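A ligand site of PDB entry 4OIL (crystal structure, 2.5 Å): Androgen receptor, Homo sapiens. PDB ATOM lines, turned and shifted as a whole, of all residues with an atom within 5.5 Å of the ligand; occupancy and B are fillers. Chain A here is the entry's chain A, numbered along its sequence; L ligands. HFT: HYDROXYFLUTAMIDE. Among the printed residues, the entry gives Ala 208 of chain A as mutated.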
ATOM      1  N   LEU A  32       5.863  23.623  31.483  1.00  0.00           N
ATOM      2  CA  LEU A  32       5.853  23.102  30.129  1.00  0.00           C
ATOM      3  C   LEU A  32       7.068  22.219  29.793  1.00  0.00           C
ATOM      4  O   LEU A  32       6.920  21.213  29.073  1.00  0.00           O
ATOM      5  CB  LEU A  32       5.645  24.209  29.127  1.00  0.00           C
ATOM      6  CG  LEU A  32       4.121  24.359  28.856  1.00  0.00           C
ATOM      7  CD1 LEU A  32       3.544  23.074  28.264  1.00  0.00           C
ATOM      8  CD2 LEU A  32       3.316  24.753  30.102  1.00  0.00           C
ATOM      9  N   LEU A  35       6.054  18.927  31.466  1.00  0.00           N
ATOM     10  CA  LEU A  35       5.030  18.161  30.650  1.00  0.00           C
ATOM     11  C   LEU A  35       5.615  17.503  29.454  1.00  0.00           C
ATOM     12  O   LEU A  35       5.225  16.414  29.123  1.00  0.00           O
ATOM     13  CB  LEU A  35       3.864  19.033  30.161  1.00  0.00           C
ATOM     14  CG  LEU A  35       2.681  19.250  31.123  1.00  0.00           C
ATOM     15  CD1 LEU A  35       1.811  20.388  30.663  1.00  0.00           C
ATOM     16  CD2 LEU A  35       1.795  18.006  31.307  1.00  0.00           C
ATOM     17  N   ASN A  36       6.485  18.226  28.744  1.00  0.00           N
ATOM     18  CA  ASN A  36       7.249  17.679  27.600  1.00  0.00           C
ATOM     19  C   ASN A  36       8.108  16.479  27.957  1.00  0.00           C
ATOM     20  O   ASN A  36       8.058  15.444  27.299  1.00  0.00           O
ATOM     21  CB  ASN A  36       8.139  18.754  26.993  1.00  0.00           C
ATOM     22  CG  ASN A  36       7.343  19.786  26.245  1.00  0.00           C
ATOM     23  OD1 ASN A  36       6.173  19.596  25.954  1.00  0.00           O
ATOM     24  ND2 ASN A  36       7.977  20.901  25.941  1.00  0.00           N
ATOM     25  N   LEU A  38       7.611  14.559  30.621  1.00  0.00           N
ATOM     26  CA  LEU A  38       6.581  13.546  30.924  1.00  0.00           C
ATOM     27  C   LEU A  38       6.060  12.937  29.629  1.00  0.00           C
ATOM     28  O   LEU A  38       5.948  11.696  29.508  1.00  0.00           O
ATOM     29  CB  LEU A  38       5.435  14.147  31.778  1.00  0.00           C
ATOM     30  CG  LEU A  38       4.308  13.171  32.137  1.00  0.00           C
ATOM     31  CD1 LEU A  38       4.869  12.007  32.951  1.00  0.00           C
ATOM     32  CD2 LEU A  38       3.152  13.855  32.845  1.00  0.00           C
ATOM     33  N   GLY A  39       5.830  13.779  28.634  1.00  0.00           N
ATOM     34  CA  GLY A  39       5.310  13.286  27.379  1.00  0.00           C
ATOM     35  C   GLY A  39       6.183  12.183  26.812  1.00  0.00           C
ATOM     36  O   GLY A  39       5.696  11.138  26.385  1.00  0.00           O
ATOM     37  N   GLN A  42       6.075   9.060  28.777  1.00  0.00           N
ATOM     38  CA  GLN A  42       4.820   8.300  28.583  1.00  0.00           C
ATOM     39  C   GLN A  42       4.771   7.697  27.180  1.00  0.00           C
ATOM     40  O   GLN A  42       4.291   6.572  26.996  1.00  0.00           O
ATOM     41  CB  GLN A  42       3.567   9.158  28.915  1.00  0.00           C
ATOM     42  CG  GLN A  42       3.427   9.533  30.388  1.00  0.00           C
ATOM     43  CD  GLN A  42       2.021   9.969  30.840  1.00  0.00           C
ATOM     44  OE1 GLN A  42       1.842  10.350  32.015  1.00  0.00           O
ATOM     45  NE2 GLN A  42       1.037   9.901  29.951  1.00  0.00           N
ATOM     46  N   TRP A  72      -1.183   8.679  20.163  1.00  0.00           N
ATOM     47  CA  TRP A  72      -0.563   8.918  21.481  1.00  0.00           C
ATOM     48  C   TRP A  72      -1.147  10.037  22.332  1.00  0.00           C
ATOM     49  O   TRP A  72      -1.356   9.876  23.530  1.00  0.00           O
ATOM     50  CB  TRP A  72       0.953   9.105  21.323  1.00  0.00           C
ATOM     51  CG  TRP A  72       1.365  10.461  21.113  1.00  0.00           C
ATOM     52  CD1 TRP A  72       1.043  11.284  20.053  1.00  0.00           C
ATOM     53  CD2 TRP A  72       2.183  11.211  21.970  1.00  0.00           C
ATOM     54  NE1 TRP A  72       1.638  12.518  20.223  1.00  0.00           N
ATOM     55  CE2 TRP A  72       2.350  12.497  21.399  1.00  0.00           C
ATOM     56  CE3 TRP A  72       2.825  10.925  23.170  1.00  0.00           C
ATOM     57  CZ2 TRP A  72       3.115  13.490  22.000  1.00  0.00           C
ATOM     58  CZ3 TRP A  72       3.599  11.920  23.769  1.00  0.00           C
ATOM     59  CH2 TRP A  72       3.725  13.183  23.181  1.00  0.00           C
ATOM     60  N   MET A  73      -1.421  11.180  21.767  1.00  0.00           N
ATOM     61  CA  MET A  73      -1.955  12.286  22.599  1.00  0.00           C
ATOM     62  C   MET A  73      -3.308  11.866  23.219  1.00  0.00           C
ATOM     63  O   MET A  73      -3.533  12.042  24.423  1.00  0.00           O
ATOM     64  CB  MET A  73      -2.109  13.571  21.797  1.00  0.00           C
ATOM     65  CG  MET A  73      -2.631  14.757  22.595  1.00  0.00           C
ATOM     66  SD  MET A  73      -1.432  15.252  23.850  1.00  0.00           S
ATOM     67  CE  MET A  73      -0.324  16.082  22.696  1.00  0.00           C
ATOM     68  N   MET A  76      -3.004   9.263  26.108  1.00  0.00           N
ATOM     69  CA  MET A  76      -2.504   9.987  27.272  1.00  0.00           C
ATOM     70  C   MET A  76      -3.577  10.752  27.990  1.00  0.00           C
ATOM     71  O   MET A  76      -3.618  10.767  29.230  1.00  0.00           O
ATOM     72  CB  MET A  76      -1.457  11.016  26.858  1.00  0.00           C
ATOM     73  CG  MET A  76      -0.065  10.434  26.598  1.00  0.00           C
ATOM     74  SD  MET A  76       1.226  11.685  26.497  1.00  0.00           S
ATOM     75  CE  MET A  76       2.499  10.492  26.231  1.00  0.00           C
ATOM     76  N   VAL A  77      -4.358  11.488  27.206  1.00  0.00           N
ATOM     77  CA  VAL A  77      -5.443  12.287  27.727  1.00  0.00           C
ATOM     78  C   VAL A  77      -6.405  11.332  28.427  1.00  0.00           C
ATOM     79  O   VAL A  77      -6.884  11.601  29.560  1.00  0.00           O
ATOM     80  CB  VAL A  77      -6.183  12.971  26.582  1.00  0.00           C
ATOM     81  CG1 VAL A  77      -7.513  13.509  27.078  1.00  0.00           C
ATOM     82  CG2 VAL A  77      -5.359  14.107  25.999  1.00  0.00           C
ATOM     83  N   PHE A  78      -6.653  10.206  27.789  1.00  0.00           N
ATOM     84  CA  PHE A  78      -7.669   9.308  28.304  1.00  0.00           C
ATOM     85  C   PHE A  78      -7.218   8.758  29.650  1.00  0.00           C
ATOM     86  O   PHE A  78      -7.982   8.800  30.626  1.00  0.00           O
ATOM     87  CB  PHE A  78      -7.947   8.147  27.324  1.00  0.00           C
ATOM     88  CG  PHE A  78      -9.230   7.416  27.594  1.00  0.00           C
ATOM     89  CD1 PHE A  78     -10.469   8.076  27.475  1.00  0.00           C
ATOM     90  CD2 PHE A  78      -9.224   6.093  27.917  1.00  0.00           C
ATOM     91  CE1 PHE A  78     -11.654   7.412  27.712  1.00  0.00           C
ATOM     92  CE2 PHE A  78     -10.404   5.419  28.174  1.00  0.00           C
ATOM     93  CZ  PHE A  78     -11.619   6.065  28.062  1.00  0.00           C
ATOM     94  N   MET A  80      -4.937   9.817  31.552  1.00  0.00           N
ATOM     95  CA  MET A  80      -4.743  10.886  32.507  1.00  0.00           C
ATOM     96  C   MET A  80      -6.119  11.228  33.099  1.00  0.00           C
ATOM     97  O   MET A  80      -6.239  11.380  34.298  1.00  0.00           O
ATOM     98  CB  MET A  80      -4.094  12.099  31.872  1.00  0.00           C
ATOM     99  CG  MET A  80      -3.634  13.127  32.894  1.00  0.00           C
ATOM    100  SD  MET A  80      -4.832  14.390  33.499  1.00  0.00           S
ATOM    101  CE  MET A  80      -4.834  15.544  32.160  1.00  0.00           C
ATOM    102  N   ARG A  83      -6.685   8.521  35.719  1.00  0.00           N
ATOM    103  CA  ARG A  83      -5.758   8.722  36.840  1.00  0.00           C
ATOM    104  C   ARG A  83      -6.324   9.829  37.723  1.00  0.00           C
ATOM    105  O   ARG A  83      -6.303   9.727  38.931  1.00  0.00           O
ATOM    106  CB  ARG A  83      -4.359   9.156  36.366  1.00  0.00           C
ATOM    107  CG  ARG A  83      -3.410   8.043  36.022  1.00  0.00           C
ATOM    108  CD  ARG A  83      -1.922   8.472  36.063  1.00  0.00           C
ATOM    109  NE  ARG A  83      -1.612   9.678  35.265  1.00  0.00           N
ATOM    110  CZ  ARG A  83      -1.465   9.688  33.947  1.00  0.00           C
ATOM    111  NH1 ARG A  83      -1.636   8.576  33.243  1.00  0.00           N
ATOM    112  NH2 ARG A  83      -1.222  10.864  33.312  1.00  0.00           N
ATOM    113  N   PHE A  95      -1.600  14.616  36.140  1.00  0.00           N
ATOM    114  CA  PHE A  95      -0.592  14.320  35.115  1.00  0.00           C
ATOM    115  C   PHE A  95       0.441  13.296  35.602  1.00  0.00           C
ATOM    116  O   PHE A  95       0.701  12.292  34.918  1.00  0.00           O
ATOM    117  CB  PHE A  95       0.054  15.609  34.734  1.00  0.00           C
ATOM    118  CG  PHE A  95      -0.813  16.481  33.873  1.00  0.00           C
ATOM    119  CD1 PHE A  95      -1.348  17.640  34.370  1.00  0.00           C
ATOM    120  CD2 PHE A  95      -1.075  16.151  32.589  1.00  0.00           C
ATOM    121  CE1 PHE A  95      -2.056  18.483  33.565  1.00  0.00           C
ATOM    122  CE2 PHE A  95      -1.792  16.992  31.786  1.00  0.00           C
ATOM    123  CZ  PHE A  95      -2.261  18.170  32.264  1.00  0.00           C
ATOM    124  N   MET A 111      -2.800  26.388  29.364  1.00  0.00           N
ATOM    125  CA  MET A 111      -3.632  25.365  28.766  1.00  0.00           C
ATOM    126  C   MET A 111      -4.948  25.275  29.504  1.00  0.00           C
ATOM    127  O   MET A 111      -5.481  24.156  29.690  1.00  0.00           O
ATOM    128  CB  MET A 111      -2.937  24.022  28.858  1.00  0.00           C
ATOM    129  CG  MET A 111      -1.463  24.074  28.541  1.00  0.00           C
ATOM    130  SD  MET A 111      -0.611  22.480  28.676  1.00  0.00           S
ATOM    131  CE  MET A 111      -1.936  21.293  28.488  1.00  0.00           C
ATOM    132  N   MET A 118     -10.366  18.528  29.805  1.00  0.00           N
ATOM    133  CA  MET A 118      -9.913  17.257  30.348  1.00  0.00           C
ATOM    134  C   MET A 118     -10.480  17.012  31.711  1.00  0.00           C
ATOM    135  O   MET A 118     -10.694  15.845  32.078  1.00  0.00           O
ATOM    136  CB  MET A 118      -8.375  17.147  30.402  1.00  0.00           C
ATOM    137  CG  MET A 118      -7.700  16.999  29.040  1.00  0.00           C
ATOM    138  SD  MET A 118      -5.873  16.967  29.161  1.00  0.00           S
ATOM    139  CE  MET A 118      -5.526  18.697  29.317  1.00  0.00           C
ATOM    140  N   LEU A 204      -4.964  19.782  21.983  1.00  0.00           N
ATOM    141  CA  LEU A 204      -3.664  19.621  22.578  1.00  0.00           C
ATOM    142  C   LEU A 204      -2.590  19.586  21.507  1.00  0.00           C
ATOM    143  O   LEU A 204      -1.513  20.167  21.660  1.00  0.00           O
ATOM    144  CB  LEU A 204      -3.639  18.376  23.437  1.00  0.00           C
ATOM    145  CG  LEU A 204      -4.361  18.609  24.778  1.00  0.00           C
ATOM    146  CD1 LEU A 204      -4.926  17.323  25.311  1.00  0.00           C
ATOM    147  CD2 LEU A 204      -3.415  19.257  25.797  1.00  0.00           C
ATOM    148  N   PHE A 207      -1.874  23.202  20.455  1.00  0.00           N
ATOM    149  CA  PHE A 207      -1.087  23.855  21.509  1.00  0.00           C
ATOM    150  C   PHE A 207       0.394  23.479  21.490  1.00  0.00           C
ATOM    151  O   PHE A 207       1.275  24.336  21.634  1.00  0.00           O
ATOM    152  CB  PHE A 207      -1.660  23.522  22.875  1.00  0.00           C
ATOM    153  CG  PHE A 207      -0.893  24.118  23.998  1.00  0.00           C
ATOM    154  CD1 PHE A 207       0.043  23.394  24.684  1.00  0.00           C
ATOM    155  CD2 PHE A 207      -1.108  25.446  24.357  1.00  0.00           C
ATOM    156  CE1 PHE A 207       0.759  23.961  25.732  1.00  0.00           C
ATOM    157  CE2 PHE A 207      -0.393  26.026  25.408  1.00  0.00           C
ATOM    158  CZ  PHE A 207       0.544  25.283  26.084  1.00  0.00           C
ATOM    159  N   ALA A 208       0.628  22.176  21.357  1.00  0.00           N
ATOM    160  CA  ALA A 208       1.958  21.590  21.366  1.00  0.00           C
ATOM    161  C   ALA A 208       2.738  21.991  20.105  1.00  0.00           C
ATOM    162  O   ALA A 208       3.868  22.462  20.185  1.00  0.00           O
ATOM    163  CB  ALA A 208       1.841  20.088  21.446  1.00  0.00           C
ATOM    164  N   LEU A 211       3.528  25.626  20.307  1.00  0.00           N
ATOM    165  CA  LEU A 211       4.575  25.767  21.311  1.00  0.00           C
ATOM    166  C   LEU A 211       5.947  25.319  20.784  1.00  0.00           C
ATOM    167  O   LEU A 211       6.951  25.948  21.070  1.00  0.00           O
ATOM    168  CB  LEU A 211       4.187  24.972  22.550  1.00  0.00           C
ATOM    169  CG  LEU A 211       5.144  25.075  23.751  1.00  0.00           C
ATOM    170  CD1 LEU A 211       5.252  26.519  24.220  1.00  0.00           C
ATOM    171  CD2 LEU A 211       4.679  24.168  24.878  1.00  0.00           C
ATOM    172  N   PHE A 222      12.337  20.959  24.427  1.00  0.00           N
ATOM    173  CA  PHE A 222      11.662  19.813  23.805  1.00  0.00           C
ATOM    174  C   PHE A 222      12.553  18.593  23.617  1.00  0.00           C
ATOM    175  O   PHE A 222      13.465  18.608  22.809  1.00  0.00           O
ATOM    176  CB  PHE A 222      11.100  20.181  22.440  1.00  0.00           C
ATOM    177  CG  PHE A 222       9.698  20.704  22.495  1.00  0.00           C
ATOM    178  CD1 PHE A 222       9.465  22.069  22.681  1.00  0.00           C
ATOM    179  CD2 PHE A 222       8.613  19.845  22.358  1.00  0.00           C
ATOM    180  CE1 PHE A 222       8.171  22.561  22.737  1.00  0.00           C
ATOM    181  CE2 PHE A 222       7.308  20.329  22.408  1.00  0.00           C
ATOM    182  CZ  PHE A 222       7.087  21.681  22.590  1.00  0.00           C
ATOM    183  N   MET A 226       9.893  14.190  20.872  1.00  0.00           N
ATOM    184  CA  MET A 226       8.727  15.054  20.908  1.00  0.00           C
ATOM    185  C   MET A 226       8.770  15.979  19.743  1.00  0.00           C
ATOM    186  O   MET A 226       7.835  16.051  18.945  1.00  0.00           O
ATOM    187  CB  MET A 226       8.704  15.938  22.151  1.00  0.00           C
ATOM    188  CG  MET A 226       8.547  15.174  23.433  1.00  0.00           C
ATOM    189  SD  MET A 226       6.961  14.362  23.294  1.00  0.00           S
ATOM    190  CE  MET A 226       5.993  15.729  23.938  1.00  0.00           C
ATOM    191  N   ILE A 230       5.852  15.978  16.923  1.00  0.00           N
ATOM    192  CA  ILE A 230       5.090  17.180  16.853  1.00  0.00           C
ATOM    193  C   ILE A 230       5.284  17.932  15.540  1.00  0.00           C
ATOM    194  O   ILE A 230       4.417  18.698  15.138  1.00  0.00           O
ATOM    195  CB  ILE A 230       5.460  18.099  18.024  1.00  0.00           C
ATOM    196  CG1 ILE A 230       4.916  17.458  19.313  1.00  0.00           C
ATOM    197  CG2 ILE A 230       4.913  19.506  17.787  1.00  0.00           C
ATOM    198  CD1 ILE A 230       5.382  18.056  20.633  1.00  0.00           C
HETATM  199  F1  HFT L   1      -2.621  15.871  27.761  1.00  0.00           F
HETATM  200  C7  HFT L   1      -2.211  14.851  28.485  1.00  0.00           C
HETATM  201  F2  HFT L   1      -2.636  13.767  27.870  1.00  0.00           F
HETATM  202  F3  HFT L   1      -2.796  14.873  29.683  1.00  0.00           F
HETATM  203  C3  HFT L   1      -0.686  14.896  28.639  1.00  0.00           C
HETATM  204  C2  HFT L   1       0.042  15.816  27.875  1.00  0.00           C
HETATM  205  C4  HFT L   1       0.072  14.020  29.574  1.00  0.00           C
HETATM  206  N1  HFT L   1      -0.513  13.021  30.384  1.00  0.00           N
HETATM  207  O2  HFT L   1       0.263  12.342  31.287  1.00  0.00           O
HETATM  208  O1  HFT L   1      -1.681  12.657  30.292  1.00  0.00           O
HETATM  209  C5  HFT L   1       1.475  14.163  29.595  1.00  0.00           C
HETATM  210  C6  HFT L   1       2.166  15.091  28.803  1.00  0.00           C
HETATM  211  C1  HFT L   1       1.459  15.916  27.937  1.00  0.00           C
HETATM  212  N9  HFT L   1       2.178  16.787  27.196  1.00  0.00           N
HETATM  213  C10 HFT L   1       1.712  17.661  26.285  1.00  0.00           C
HETATM  214  O10 HFT L   1       0.545  17.786  25.927  1.00  0.00           O
HETATM  215  C11 HFT L   1       2.694  18.566  25.596  1.00  0.00           C
HETATM  216  C12 HFT L   1       3.473  17.959  24.431  1.00  0.00           C
HETATM  217  C13 HFT L   1       2.906  19.978  26.103  1.00  0.00           C
HETATM  218  O11 HFT L   1       3.806  18.190  26.497  1.00  0.00           O
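O2 of the ligand sits close to OE1 of Gln 42 (2.6 Å). The guanidinium group (NH2) of Arg 83 is in hydrogen-bond range of an oxygen (O2) of the ligand, 2.9 Å away. OD1 of Asn 36 sits at hydrogen-bond distance from O11 of the ligand. The backbone NH (N) of Asn 36 sits at hydrogen-bond distance from an oxygen (O11) of the ligand. The backbone carbonyl oxygen (O) of Leu 35 sits close to an oxygen (O11) of the ligand, at 3.5 Å.
O of Met 76 lies close to O1 of the ligand (2.9 Å). N of Val 77 sits close to F2 of the ligand. A fluorine (F1) of the ligand lies close to the side-chain sulfur (SD) of Met 118. Residues that only touch the ligand: Leu 32, Leu 38, Gly 39, Met 73, Met 80, Phe 95, Leu 204 and Met 226. Within 4 Å of the ligand: Leu 32, Leu 35, Asn 36, Leu 38, Gly 39, Gln 42, Met 73, Met 76, Val 77, Met 80, Arg 83, Phe 95, Met 118, Leu 204 and Met 226. Along chain A the residues within 4 Å of the ligand span positions 32 to 226. The nearest printed residue that does not touch the ligand is Ala 208 (4.01 Å).
The backbone carbonyl oxygen (O) of Leu 32 lies close to the side-chain amide nitrogen (ND2) of Asn 36 (3.3 Å). NH2 of Arg 83 lies within hydrogen-bond range of O of Phe 95 (2.9 Å). The side-chain amide oxygen (OE1) of Gln 42 is in hydrogen-bond range of the guanidinium group (NH2) of Arg 83, 3.4 Å away.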
